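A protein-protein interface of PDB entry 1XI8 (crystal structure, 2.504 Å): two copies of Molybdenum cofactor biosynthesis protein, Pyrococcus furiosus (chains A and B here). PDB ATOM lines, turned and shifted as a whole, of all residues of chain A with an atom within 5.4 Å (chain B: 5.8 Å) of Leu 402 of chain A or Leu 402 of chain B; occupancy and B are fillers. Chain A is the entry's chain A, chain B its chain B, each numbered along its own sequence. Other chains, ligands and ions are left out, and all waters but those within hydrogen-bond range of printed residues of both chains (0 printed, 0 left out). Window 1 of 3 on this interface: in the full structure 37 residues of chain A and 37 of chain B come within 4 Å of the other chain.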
ATOM      1  N   TYR A 230     -12.009 -15.087  22.761  1.00  0.00           N
ATOM      2  CA  TYR A 230     -11.492 -14.110  21.799  1.00  0.00           C
ATOM      3  C   TYR A 230     -11.584 -12.650  22.234  1.00  0.00           C
ATOM      4  O   TYR A 230     -12.207 -11.827  21.572  1.00  0.00           O
ATOM      5  CB  TYR A 230     -12.081 -14.337  20.393  1.00  0.00           C
ATOM      6  CG  TYR A 230     -11.532 -15.591  19.765  1.00  0.00           C
ATOM      7  CD1 TYR A 230     -10.263 -15.611  19.203  1.00  0.00           C
ATOM      8  CD2 TYR A 230     -12.267 -16.765  19.768  1.00  0.00           C
ATOM      9  CE1 TYR A 230      -9.745 -16.760  18.643  1.00  0.00           C
ATOM     10  CE2 TYR A 230     -11.763 -17.921  19.214  1.00  0.00           C
ATOM     11  CZ  TYR A 230     -10.501 -17.915  18.653  1.00  0.00           C
ATOM     12  OH  TYR A 230     -10.012 -19.076  18.099  1.00  0.00           O
ATOM     13  N   HIS A 315     -16.868 -17.285  14.026  1.00  0.00           N
ATOM     14  CA  HIS A 315     -15.526 -17.452  13.467  1.00  0.00           C
ATOM     15  C   HIS A 315     -15.289 -16.692  12.162  1.00  0.00           C
ATOM     16  O   HIS A 315     -14.187 -16.204  11.922  1.00  0.00           O
ATOM     17  CB  HIS A 315     -15.183 -18.934  13.286  1.00  0.00           C
ATOM     18  CG  HIS A 315     -14.788 -19.614  14.559  1.00  0.00           C
ATOM     19  ND1 HIS A 315     -13.500 -19.588  15.048  1.00  0.00           N
ATOM     20  CD2 HIS A 315     -15.513 -20.332  15.451  1.00  0.00           C
ATOM     21  CE1 HIS A 315     -13.448 -20.261  16.180  1.00  0.00           C
ATOM     22  NE2 HIS A 315     -14.655 -20.722  16.447  1.00  0.00           N
ATOM     23  N   LYS A 319     -15.239 -13.030  15.725  1.00  0.00           N
ATOM     24  CA  LYS A 319     -13.843 -13.208  16.113  1.00  0.00           C
ATOM     25  C   LYS A 319     -12.935 -12.132  15.498  1.00  0.00           C
ATOM     26  O   LYS A 319     -12.039 -11.608  16.160  1.00  0.00           O
ATOM     27  CB  LYS A 319     -13.374 -14.593  15.687  1.00  0.00           C
ATOM     28  CG  LYS A 319     -11.929 -14.908  15.996  1.00  0.00           C
ATOM     29  CD  LYS A 319     -11.568 -16.356  15.612  1.00  0.00           C
ATOM     30  CE  LYS A 319     -11.609 -16.585  14.099  1.00  0.00           C
ATOM     31  NZ  LYS A 319     -11.067 -17.912  13.681  1.00  0.00           N
ATOM     32  N   VAL A 333      -4.275 -19.705  13.455  1.00  0.00           N
ATOM     33  CA  VAL A 333      -3.263 -20.593  12.919  1.00  0.00           C
ATOM     34  C   VAL A 333      -3.859 -21.400  11.756  1.00  0.00           C
ATOM     35  O   VAL A 333      -4.784 -22.201  11.964  1.00  0.00           O
ATOM     36  CB  VAL A 333      -2.778 -21.608  13.994  1.00  0.00           C
ATOM     37  CG1 VAL A 333      -1.488 -22.296  13.543  1.00  0.00           C
ATOM     38  CG2 VAL A 333      -2.590 -20.956  15.376  1.00  0.00           C
ATOM     39  N   LYS A 334      -3.337 -21.180  10.544  1.00  0.00           N
ATOM     40  CA  LYS A 334      -3.630 -22.014   9.382  1.00  0.00           C
ATOM     41  C   LYS A 334      -2.627 -23.173   9.357  1.00  0.00           C
ATOM     42  O   LYS A 334      -1.429 -22.969   9.579  1.00  0.00           O
ATOM     43  CB  LYS A 334      -3.428 -21.248   8.075  1.00  0.00           C
ATOM     44  CG  LYS A 334      -4.488 -20.244   7.672  1.00  0.00           C
ATOM     45  CD  LYS A 334      -4.528 -20.072   6.135  1.00  0.00           C
ATOM     46  CE  LYS A 334      -3.270 -19.416   5.565  1.00  0.00           C
ATOM     47  NZ  LYS A 334      -3.365 -19.242   4.068  1.00  0.00           N
ATOM     48  N   VAL A 335      -3.105 -24.382   9.072  1.00  0.00           N
ATOM     49  CA  VAL A 335      -2.205 -25.517   8.899  1.00  0.00           C
ATOM     50  C   VAL A 335      -2.515 -26.258   7.607  1.00  0.00           C
ATOM     51  O   VAL A 335      -3.619 -26.167   7.088  1.00  0.00           O
ATOM     52  CB  VAL A 335      -2.235 -26.501  10.100  1.00  0.00           C
ATOM     53  CG1 VAL A 335      -2.038 -25.752  11.407  1.00  0.00           C
ATOM     54  CG2 VAL A 335      -3.523 -27.301  10.130  1.00  0.00           C
ATOM     55  N   TYR A 357      -8.702 -32.056  12.790  1.00  0.00           N
ATOM     56  CA  TYR A 357      -7.321 -32.038  12.370  1.00  0.00           C
ATOM     57  C   TYR A 357      -6.419 -32.747  13.348  1.00  0.00           C
ATOM     58  O   TYR A 357      -6.410 -32.430  14.537  1.00  0.00           O
ATOM     59  CB  TYR A 357      -6.786 -30.611  12.182  1.00  0.00           C
ATOM     60  CG  TYR A 357      -5.292 -30.639  11.998  1.00  0.00           C
ATOM     61  CD1 TYR A 357      -4.728 -30.868  10.739  1.00  0.00           C
ATOM     62  CD2 TYR A 357      -4.440 -30.490  13.085  1.00  0.00           C
ATOM     63  CE1 TYR A 357      -3.362 -30.919  10.574  1.00  0.00           C
ATOM     64  CE2 TYR A 357      -3.072 -30.541  12.928  1.00  0.00           C
ATOM     65  CZ  TYR A 357      -2.538 -30.754  11.675  1.00  0.00           C
ATOM     66  OH  TYR A 357      -1.174 -30.796  11.532  1.00  0.00           O
ATOM     67  N   ASN A 380     -12.153 -29.631  15.451  1.00  0.00           N
ATOM     68  CA  ASN A 380     -11.173 -28.783  16.143  1.00  0.00           C
ATOM     69  C   ASN A 380     -10.624 -27.702  15.205  1.00  0.00           C
ATOM     70  O   ASN A 380      -9.742 -26.913  15.569  1.00  0.00           O
ATOM     71  CB  ASN A 380     -10.014 -29.626  16.675  1.00  0.00           C
ATOM     72  CG  ASN A 380      -9.191 -30.275  15.556  1.00  0.00           C
ATOM     73  OD1 ASN A 380      -9.537 -30.189  14.374  1.00  0.00           O
ATOM     74  ND2 ASN A 380      -8.099 -30.926  15.930  1.00  0.00           N
ATOM     75  N   ALA A 381     -11.152 -27.686  13.987  1.00  0.00           N
ATOM     76  CA  ALA A 381     -10.687 -26.771  12.957  1.00  0.00           C
ATOM     77  C   ALA A 381     -11.738 -26.627  11.875  1.00  0.00           C
ATOM     78  O   ALA A 381     -12.722 -27.358  11.845  1.00  0.00           O
ATOM     79  CB  ALA A 381      -9.382 -27.269  12.354  1.00  0.00           C
ATOM     80  N   TYR A 382     -11.534 -25.670  10.987  1.00  0.00           N
ATOM     81  CA  TYR A 382     -12.467 -25.493   9.905  1.00  0.00           C
ATOM     82  C   TYR A 382     -11.761 -25.188   8.602  1.00  0.00           C
ATOM     83  O   TYR A 382     -10.684 -24.597   8.570  1.00  0.00           O
ATOM     84  CB  TYR A 382     -13.508 -24.416  10.226  1.00  0.00           C
ATOM     85  CG  TYR A 382     -12.970 -23.007  10.347  1.00  0.00           C
ATOM     86  CD1 TYR A 382     -12.577 -22.499  11.578  1.00  0.00           C
ATOM     87  CD2 TYR A 382     -12.869 -22.175   9.231  1.00  0.00           C
ATOM     88  CE1 TYR A 382     -12.098 -21.216  11.703  1.00  0.00           C
ATOM     89  CE2 TYR A 382     -12.386 -20.884   9.349  1.00  0.00           C
ATOM     90  CZ  TYR A 382     -12.003 -20.411  10.587  1.00  0.00           C
ATOM     91  OH  TYR A 382     -11.518 -19.126  10.726  1.00  0.00           O
ATOM     92  N   VAL A 400      -6.622 -25.485   6.846  1.00  0.00           N
ATOM     93  CA  VAL A 400      -7.665 -25.488   7.853  1.00  0.00           C
ATOM     94  C   VAL A 400      -7.229 -24.556   8.976  1.00  0.00           C
ATOM     95  O   VAL A 400      -6.040 -24.426   9.268  1.00  0.00           O
ATOM     96  CB  VAL A 400      -8.001 -26.912   8.395  1.00  0.00           C
ATOM     97  CG1 VAL A 400      -8.437 -27.835   7.259  1.00  0.00           C
ATOM     98  CG2 VAL A 400      -6.828 -27.504   9.153  1.00  0.00           C
ATOM     99  N   THR A 401      -8.197 -23.896   9.594  1.00  0.00           N
ATOM    100  CA  THR A 401      -7.900 -22.965  10.664  1.00  0.00           C
ATOM    101  C   THR A 401      -8.304 -23.548  12.019  1.00  0.00           C
ATOM    102  O   THR A 401      -9.457 -23.910  12.218  1.00  0.00           O
ATOM    103  CB  THR A 401      -8.572 -21.605  10.395  1.00  0.00           C
ATOM    104  OG1 THR A 401      -8.021 -21.046   9.197  1.00  0.00           O
ATOM    105  CG2 THR A 401      -8.359 -20.631  11.568  1.00  0.00           C
ATOM    106  N   LEU A 402      -7.351 -23.638  12.943  1.00  0.00           N
ATOM    107  CA  LEU A 402      -7.642 -24.202  14.261  1.00  0.00           C
ATOM    108  C   LEU A 402      -8.637 -23.342  15.033  1.00  0.00           C
ATOM    109  O   LEU A 402      -8.630 -22.122  14.926  1.00  0.00           O
ATOM    110  CB  LEU A 402      -6.367 -24.406  15.085  1.00  0.00           C
ATOM    111  CG  LEU A 402      -5.244 -25.234  14.458  1.00  0.00           C
ATOM    112  CD1 LEU A 402      -3.995 -25.158  15.331  1.00  0.00           C
ATOM    113  CD2 LEU A 402      -5.651 -26.675  14.216  1.00  0.00           C
ATOM    114  N   TYR A 403      -9.498 -23.991  15.803  1.00  0.00           N
ATOM    115  CA  TYR A 403     -10.440 -23.279  16.651  1.00  0.00           C
ATOM    116  C   TYR A 403      -9.669 -22.567  17.750  1.00  0.00           C
ATOM    117  O   TYR A 403     -10.229 -21.707  18.426  1.00  0.00           O
ATOM    118  CB  TYR A 403     -11.463 -24.229  17.289  1.00  0.00           C
ATOM    119  CG  TYR A 403     -12.455 -24.867  16.345  1.00  0.00           C
ATOM    120  CD1 TYR A 403     -12.718 -24.316  15.089  1.00  0.00           C
ATOM    121  CD2 TYR A 403     -13.156 -26.010  16.723  1.00  0.00           C
ATOM    122  CE1 TYR A 403     -13.631 -24.901  14.237  1.00  0.00           C
ATOM    123  CE2 TYR A 403     -14.063 -26.592  15.885  1.00  0.00           C
ATOM    124  CZ  TYR A 403     -14.303 -26.040  14.647  1.00  0.00           C
ATOM    125  OH  TYR A 403     -15.213 -26.631  13.817  1.00  0.00           O
ATOM    126  N   TYR B 230      -1.487 -25.295  31.169  1.00  0.00           N
ATOM    127  CA  TYR B 230      -1.552 -26.759  31.063  1.00  0.00           C
ATOM    128  C   TYR B 230      -2.150 -27.511  32.278  1.00  0.00           C
ATOM    129  O   TYR B 230      -1.517 -28.398  32.866  1.00  0.00           O
ATOM    130  CB  TYR B 230      -0.196 -27.340  30.627  1.00  0.00           C
ATOM    131  CG  TYR B 230       0.044 -27.109  29.159  1.00  0.00           C
ATOM    132  CD1 TYR B 230      -0.594 -27.890  28.210  1.00  0.00           C
ATOM    133  CD2 TYR B 230       0.885 -26.093  28.711  1.00  0.00           C
ATOM    134  CE1 TYR B 230      -0.400 -27.675  26.859  1.00  0.00           C
ATOM    135  CE2 TYR B 230       1.089 -25.875  27.353  1.00  0.00           C
ATOM    136  CZ  TYR B 230       0.442 -26.672  26.435  1.00  0.00           C
ATOM    137  OH  TYR B 230       0.622 -26.482  25.079  1.00  0.00           O
ATOM    138  N   HIS B 315       8.075 -28.263  28.415  1.00  0.00           N
ATOM    139  CA  HIS B 315       7.406 -28.805  27.239  1.00  0.00           C
ATOM    140  C   HIS B 315       7.725 -30.269  26.926  1.00  0.00           C
ATOM    141  O   HIS B 315       6.891 -30.990  26.395  1.00  0.00           O
ATOM    142  CB  HIS B 315       7.672 -27.913  26.013  1.00  0.00           C
ATOM    143  CG  HIS B 315       6.722 -26.768  25.909  1.00  0.00           C
ATOM    144  ND1 HIS B 315       5.542 -26.847  25.207  1.00  0.00           N
ATOM    145  CD2 HIS B 315       6.749 -25.534  26.463  1.00  0.00           C
ATOM    146  CE1 HIS B 315       4.893 -25.703  25.311  1.00  0.00           C
ATOM    147  NE2 HIS B 315       5.603 -24.890  26.068  1.00  0.00           N
ATOM    148  N   LYS B 319       4.816 -30.822  31.059  1.00  0.00           N
ATOM    149  CA  LYS B 319       3.547 -30.757  30.318  1.00  0.00           C
ATOM    150  C   LYS B 319       2.859 -32.126  30.192  1.00  0.00           C
ATOM    151  O   LYS B 319       1.668 -32.272  30.480  1.00  0.00           O
ATOM    152  CB  LYS B 319       3.776 -30.162  28.925  1.00  0.00           C
ATOM    153  CG  LYS B 319       2.558 -30.192  28.015  1.00  0.00           C
ATOM    154  CD  LYS B 319       2.838 -29.585  26.639  1.00  0.00           C
ATOM    155  CE  LYS B 319       3.705 -30.503  25.772  1.00  0.00           C
ATOM    156  NZ  LYS B 319       4.069 -29.884  24.463  1.00  0.00           N
ATOM    157  N   VAL B 333      -0.813 -30.168  19.372  1.00  0.00           N
ATOM    158  CA  VAL B 333      -1.112 -30.075  17.953  1.00  0.00           C
ATOM    159  C   VAL B 333       0.209 -30.115  17.200  1.00  0.00           C
ATOM    160  O   VAL B 333       1.089 -29.282  17.433  1.00  0.00           O
ATOM    161  CB  VAL B 333      -1.886 -28.772  17.612  1.00  0.00           C
ATOM    162  CG1 VAL B 333      -2.270 -28.738  16.141  1.00  0.00           C
ATOM    163  CG2 VAL B 333      -3.128 -28.622  18.491  1.00  0.00           C
ATOM    164  N   LYS B 334       0.347 -31.102  16.320  1.00  0.00           N
ATOM    165  CA  LYS B 334       1.523 -31.245  15.471  1.00  0.00           C
ATOM    166  C   LYS B 334       1.154 -30.727  14.085  1.00  0.00           C
ATOM    167  O   LYS B 334       0.095 -31.072  13.557  1.00  0.00           O
ATOM    168  CB  LYS B 334       1.952 -32.720  15.342  1.00  0.00           C
ATOM    169  CG  LYS B 334       3.104 -33.185  16.225  1.00  0.00           C
ATOM    170  CD  LYS B 334       3.940 -34.303  15.545  1.00  0.00           C
ATOM    171  CE  LYS B 334       3.194 -35.663  15.421  1.00  0.00           C
ATOM    172  NZ  LYS B 334       4.025 -36.784  14.825  1.00  0.00           N
ATOM    173  N   VAL B 335       2.021 -29.906  13.494  1.00  0.00           N
ATOM    174  CA  VAL B 335       1.788 -29.450  12.121  1.00  0.00           C
ATOM    175  C   VAL B 335       2.980 -29.681  11.202  1.00  0.00           C
ATOM    176  O   VAL B 335       4.128 -29.687  11.641  1.00  0.00           O
ATOM    177  CB  VAL B 335       1.353 -27.974  12.059  1.00  0.00           C
ATOM    178  CG1 VAL B 335       0.291 -27.696  13.117  1.00  0.00           C
ATOM    179  CG2 VAL B 335       2.535 -27.052  12.244  1.00  0.00           C
ATOM    180  N   TYR B 357       6.287 -20.600  13.464  1.00  0.00           N
ATOM    181  CA  TYR B 357       5.547 -21.313  12.431  1.00  0.00           C
ATOM    182  C   TYR B 357       4.456 -20.440  11.844  1.00  0.00           C
ATOM    183  O   TYR B 357       3.606 -19.947  12.570  1.00  0.00           O
ATOM    184  CB  TYR B 357       4.918 -22.624  12.950  1.00  0.00           C
ATOM    185  CG  TYR B 357       3.840 -23.092  12.010  1.00  0.00           C
ATOM    186  CD1 TYR B 357       4.143 -23.876  10.896  1.00  0.00           C
ATOM    187  CD2 TYR B 357       2.514 -22.701  12.199  1.00  0.00           C
ATOM    188  CE1 TYR B 357       3.138 -24.278  10.013  1.00  0.00           C
ATOM    189  CE2 TYR B 357       1.509 -23.091  11.325  1.00  0.00           C
ATOM    190  CZ  TYR B 357       1.820 -23.877  10.241  1.00  0.00           C
ATOM    191  OH  TYR B 357       0.803 -24.249   9.391  1.00  0.00           O
ATOM    192  N   ASN B 380       6.783 -19.631  18.299  1.00  0.00           N
ATOM    193  CA  ASN B 380       5.436 -20.055  18.678  1.00  0.00           C
ATOM    194  C   ASN B 380       5.278 -21.574  18.614  1.00  0.00           C
ATOM    195  O   ASN B 380       4.185 -22.102  18.783  1.00  0.00           O
ATOM    196  CB  ASN B 380       4.381 -19.366  17.806  1.00  0.00           C
ATOM    197  CG  ASN B 380       4.475 -19.766  16.347  1.00  0.00           C
ATOM    198  OD1 ASN B 380       5.346 -20.529  15.960  1.00  0.00           O
ATOM    199  ND2 ASN B 380       3.566 -19.257  15.535  1.00  0.00           N
ATOM    200  N   ALA B 381       6.384 -22.267  18.362  1.00  0.00           N
ATOM    201  CA  ALA B 381       6.374 -23.719  18.200  1.00  0.00           C
ATOM    202  C   ALA B 381       7.768 -24.303  18.381  1.00  0.00           C
ATOM    203  O   ALA B 381       8.745 -23.562  18.490  1.00  0.00           O
ATOM    204  CB  ALA B 381       5.819 -24.101  16.831  1.00  0.00           C
ATOM    205  N   TYR B 382       7.862 -25.630  18.417  1.00  0.00           N
ATOM    206  CA  TYR B 382       9.166 -26.270  18.545  1.00  0.00           C
ATOM    207  C   TYR B 382       9.367 -27.519  17.700  1.00  0.00           C
ATOM    208  O   TYR B 382       8.479 -28.370  17.582  1.00  0.00           O
ATOM    209  CB  TYR B 382       9.506 -26.570  20.008  1.00  0.00           C
ATOM    210  CG  TYR B 382       8.654 -27.620  20.687  1.00  0.00           C
ATOM    211  CD1 TYR B 382       7.480 -27.267  21.343  1.00  0.00           C
ATOM    212  CD2 TYR B 382       9.039 -28.960  20.698  1.00  0.00           C
ATOM    213  CE1 TYR B 382       6.701 -28.210  21.981  1.00  0.00           C
ATOM    214  CE2 TYR B 382       8.271 -29.918  21.332  1.00  0.00           C
ATOM    215  CZ  TYR B 382       7.093 -29.540  21.977  1.00  0.00           C
ATOM    216  OH  TYR B 382       6.308 -30.484  22.613  1.00  0.00           O
ATOM    217  N   VAL B 400       6.503 -29.626  13.604  1.00  0.00           N
ATOM    218  CA  VAL B 400       6.694 -28.710  14.699  1.00  0.00           C
ATOM    219  C   VAL B 400       5.472 -28.836  15.616  1.00  0.00           C
ATOM    220  O   VAL B 400       4.365 -29.109  15.153  1.00  0.00           O
ATOM    221  CB  VAL B 400       6.912 -27.243  14.215  1.00  0.00           C
ATOM    222  CG1 VAL B 400       7.995 -27.177  13.134  1.00  0.00           C
ATOM    223  CG2 VAL B 400       5.626 -26.625  13.703  1.00  0.00           C
ATOM    224  N   THR B 401       5.674 -28.665  16.914  1.00  0.00           N
ATOM    225  CA  THR B 401       4.556 -28.681  17.832  1.00  0.00           C
ATOM    226  C   THR B 401       4.312 -27.271  18.351  1.00  0.00           C
ATOM    227  O   THR B 401       5.241 -26.609  18.808  1.00  0.00           O
ATOM    228  CB  THR B 401       4.779 -29.649  19.007  1.00  0.00           C
ATOM    229  OG1 THR B 401       4.769 -30.999  18.519  1.00  0.00           O
ATOM    230  CG2 THR B 401       3.677 -29.468  20.059  1.00  0.00           C
ATOM    231  N   LEU B 402       3.064 -26.815  18.271  1.00  0.00           N
ATOM    232  CA  LEU B 402       2.734 -25.454  18.666  1.00  0.00           C
ATOM    233  C   LEU B 402       2.813 -25.299  20.171  1.00  0.00           C
ATOM    234  O   LEU B 402       2.494 -26.224  20.908  1.00  0.00           O
ATOM    235  CB  LEU B 402       1.332 -25.067  18.198  1.00  0.00           C
ATOM    236  CG  LEU B 402       0.996 -25.157  16.714  1.00  0.00           C
ATOM    237  CD1 LEU B 402      -0.451 -24.760  16.502  1.00  0.00           C
ATOM    238  CD2 LEU B 402       1.929 -24.308  15.868  1.00  0.00           C
ATOM    239  N   TYR B 403       3.239 -24.124  20.624  1.00  0.00           N
ATOM    240  CA  TYR B 403       3.190 -23.824  22.045  1.00  0.00           C
ATOM    241  C   TYR B 403       1.758 -23.869  22.548  1.00  0.00           C
ATOM    242  O   TYR B 403       1.550 -24.052  23.742  1.00  0.00           O
ATOM    243  CB  TYR B 403       3.798 -22.461  22.356  1.00  0.00           C
ATOM    244  CG  TYR B 403       5.277 -22.397  22.086  1.00  0.00           C
ATOM    245  CD1 TYR B 403       6.031 -23.563  21.967  1.00  0.00           C
ATOM    246  CD2 TYR B 403       5.931 -21.178  21.967  1.00  0.00           C
ATOM    247  CE1 TYR B 403       7.384 -23.510  21.719  1.00  0.00           C
ATOM    248  CE2 TYR B 403       7.283 -21.125  21.728  1.00  0.00           C
ATOM    249  CZ  TYR B 403       8.000 -22.289  21.603  1.00  0.00           C
ATOM    250  OH  TYR B 403       9.342 -22.239  21.366  1.00  0.00           O
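Printed residues of chain B that touch a printed residue of chain A: Val 333, Lys 334, Val 335, Tyr 357 and Leu 402.
Of the 14 printed residues of chain A, 5 touch a printed residue of chain B.
Hydrophobic or aromatic side chains of chain A within 4 Å of the printed part of chain B: Val 333, Val 335, Tyr 357 and Leu 402.
Among the printed residues, 9 pairs touch across the chains.
Among the printed residues, no Asp or Glu carboxylate lies within 4 Å of a Lys or Arg side-chain nitrogen of the other chain.
Among the printed residues, merely in contact across the chains: Val 333 of chain A with Tyr 357 of chain B, Val 333 of chain A with Leu 402 of chain B, Val 335 of chain A with Val 335 of chain B, Val 335 of chain A with Tyr 357 of chain B, Tyr 357 of chain A with Val 333 of chain B, Tyr 357 of chain A with Val 335 of chain B and Leu 402 of chain A with Leu 402 of chain B.
Leu 402 of chain A touches one residue of chain B.
Printed residues of chain A within 4 Å of Leu 402 of chain B: Val 333 and Leu 402.
Printed residues of chain A within 4 Å of Val 335 of chain B: Val 335 and Tyr 357.
Printed residues of chain A within 4 Å of Tyr 357 of chain B: Val 333, Lys 334 and Val 335.
Of the printed residues of chain A, Lys 334 of chain B touches Tyr 357.
Ala 381 of chain A touches none of the printed residues of chain B.
The nearest residue of chain B that does not touch Leu 402 of chain A is Val 333 of chain B (4.1 Å).
The side-chain hydroxyl of Tyr 357 of chain A lies within hydrogen-bond range of the backbone carbonyl oxygen of Lys 334 of chain B.
The backbone carbonyl oxygen of Lys 334 of chain A sits at hydrogen-bond distance from the side-chain hydroxyl of Tyr 357 of chain B, 2.6 Å away.
N of Tyr 357 of chain A lies within hydrogen-bond range of OD1 of Asn 380 of chain A (2.6 Å).
The backbone carbonyl oxygen of Val 333 of chain B lies within hydrogen-bond range of the backbone NH of Leu 402 of chain B (3.3 Å).
The backbone NH of Tyr 357 of chain B sits at hydrogen-bond distance from the side-chain amide oxygen of Asn 380 of chain B, 2.7 Å away.
O of Val 333 of chain A lies within hydrogen-bond range of N of Leu 402 of chain A, 3.1 Å away.
The backbone NH (N) of Val 335 of chain B is in hydrogen-bond range of the backbone carbonyl oxygen (O) of Val 400 of chain B.
N of Val 335 of chain A lies within hydrogen-bond range of O of Val 400 of chain A (2.9 Å).
Val 333 of chain A touches Tyr 357 of chain B, and with the chains exchanged Tyr 357 of chain A touches Val 333 of chain B.
Val 333 of chain A touches Leu 402 of chain B, but with the chains exchanged Leu 402 of chain A does not touch Val 333 of chain B (4.1 Å).
Lys 334 of chain A touches Tyr 357 of chain B, and with the chains exchanged Tyr 357 of chain A touches Lys 334 of chain B.
Val 335 of chain A touches Tyr 357 of chain B, and with the chains exchanged Tyr 357 of chain A touches Val 335 of chain B.
14 positions are printed for both chains.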
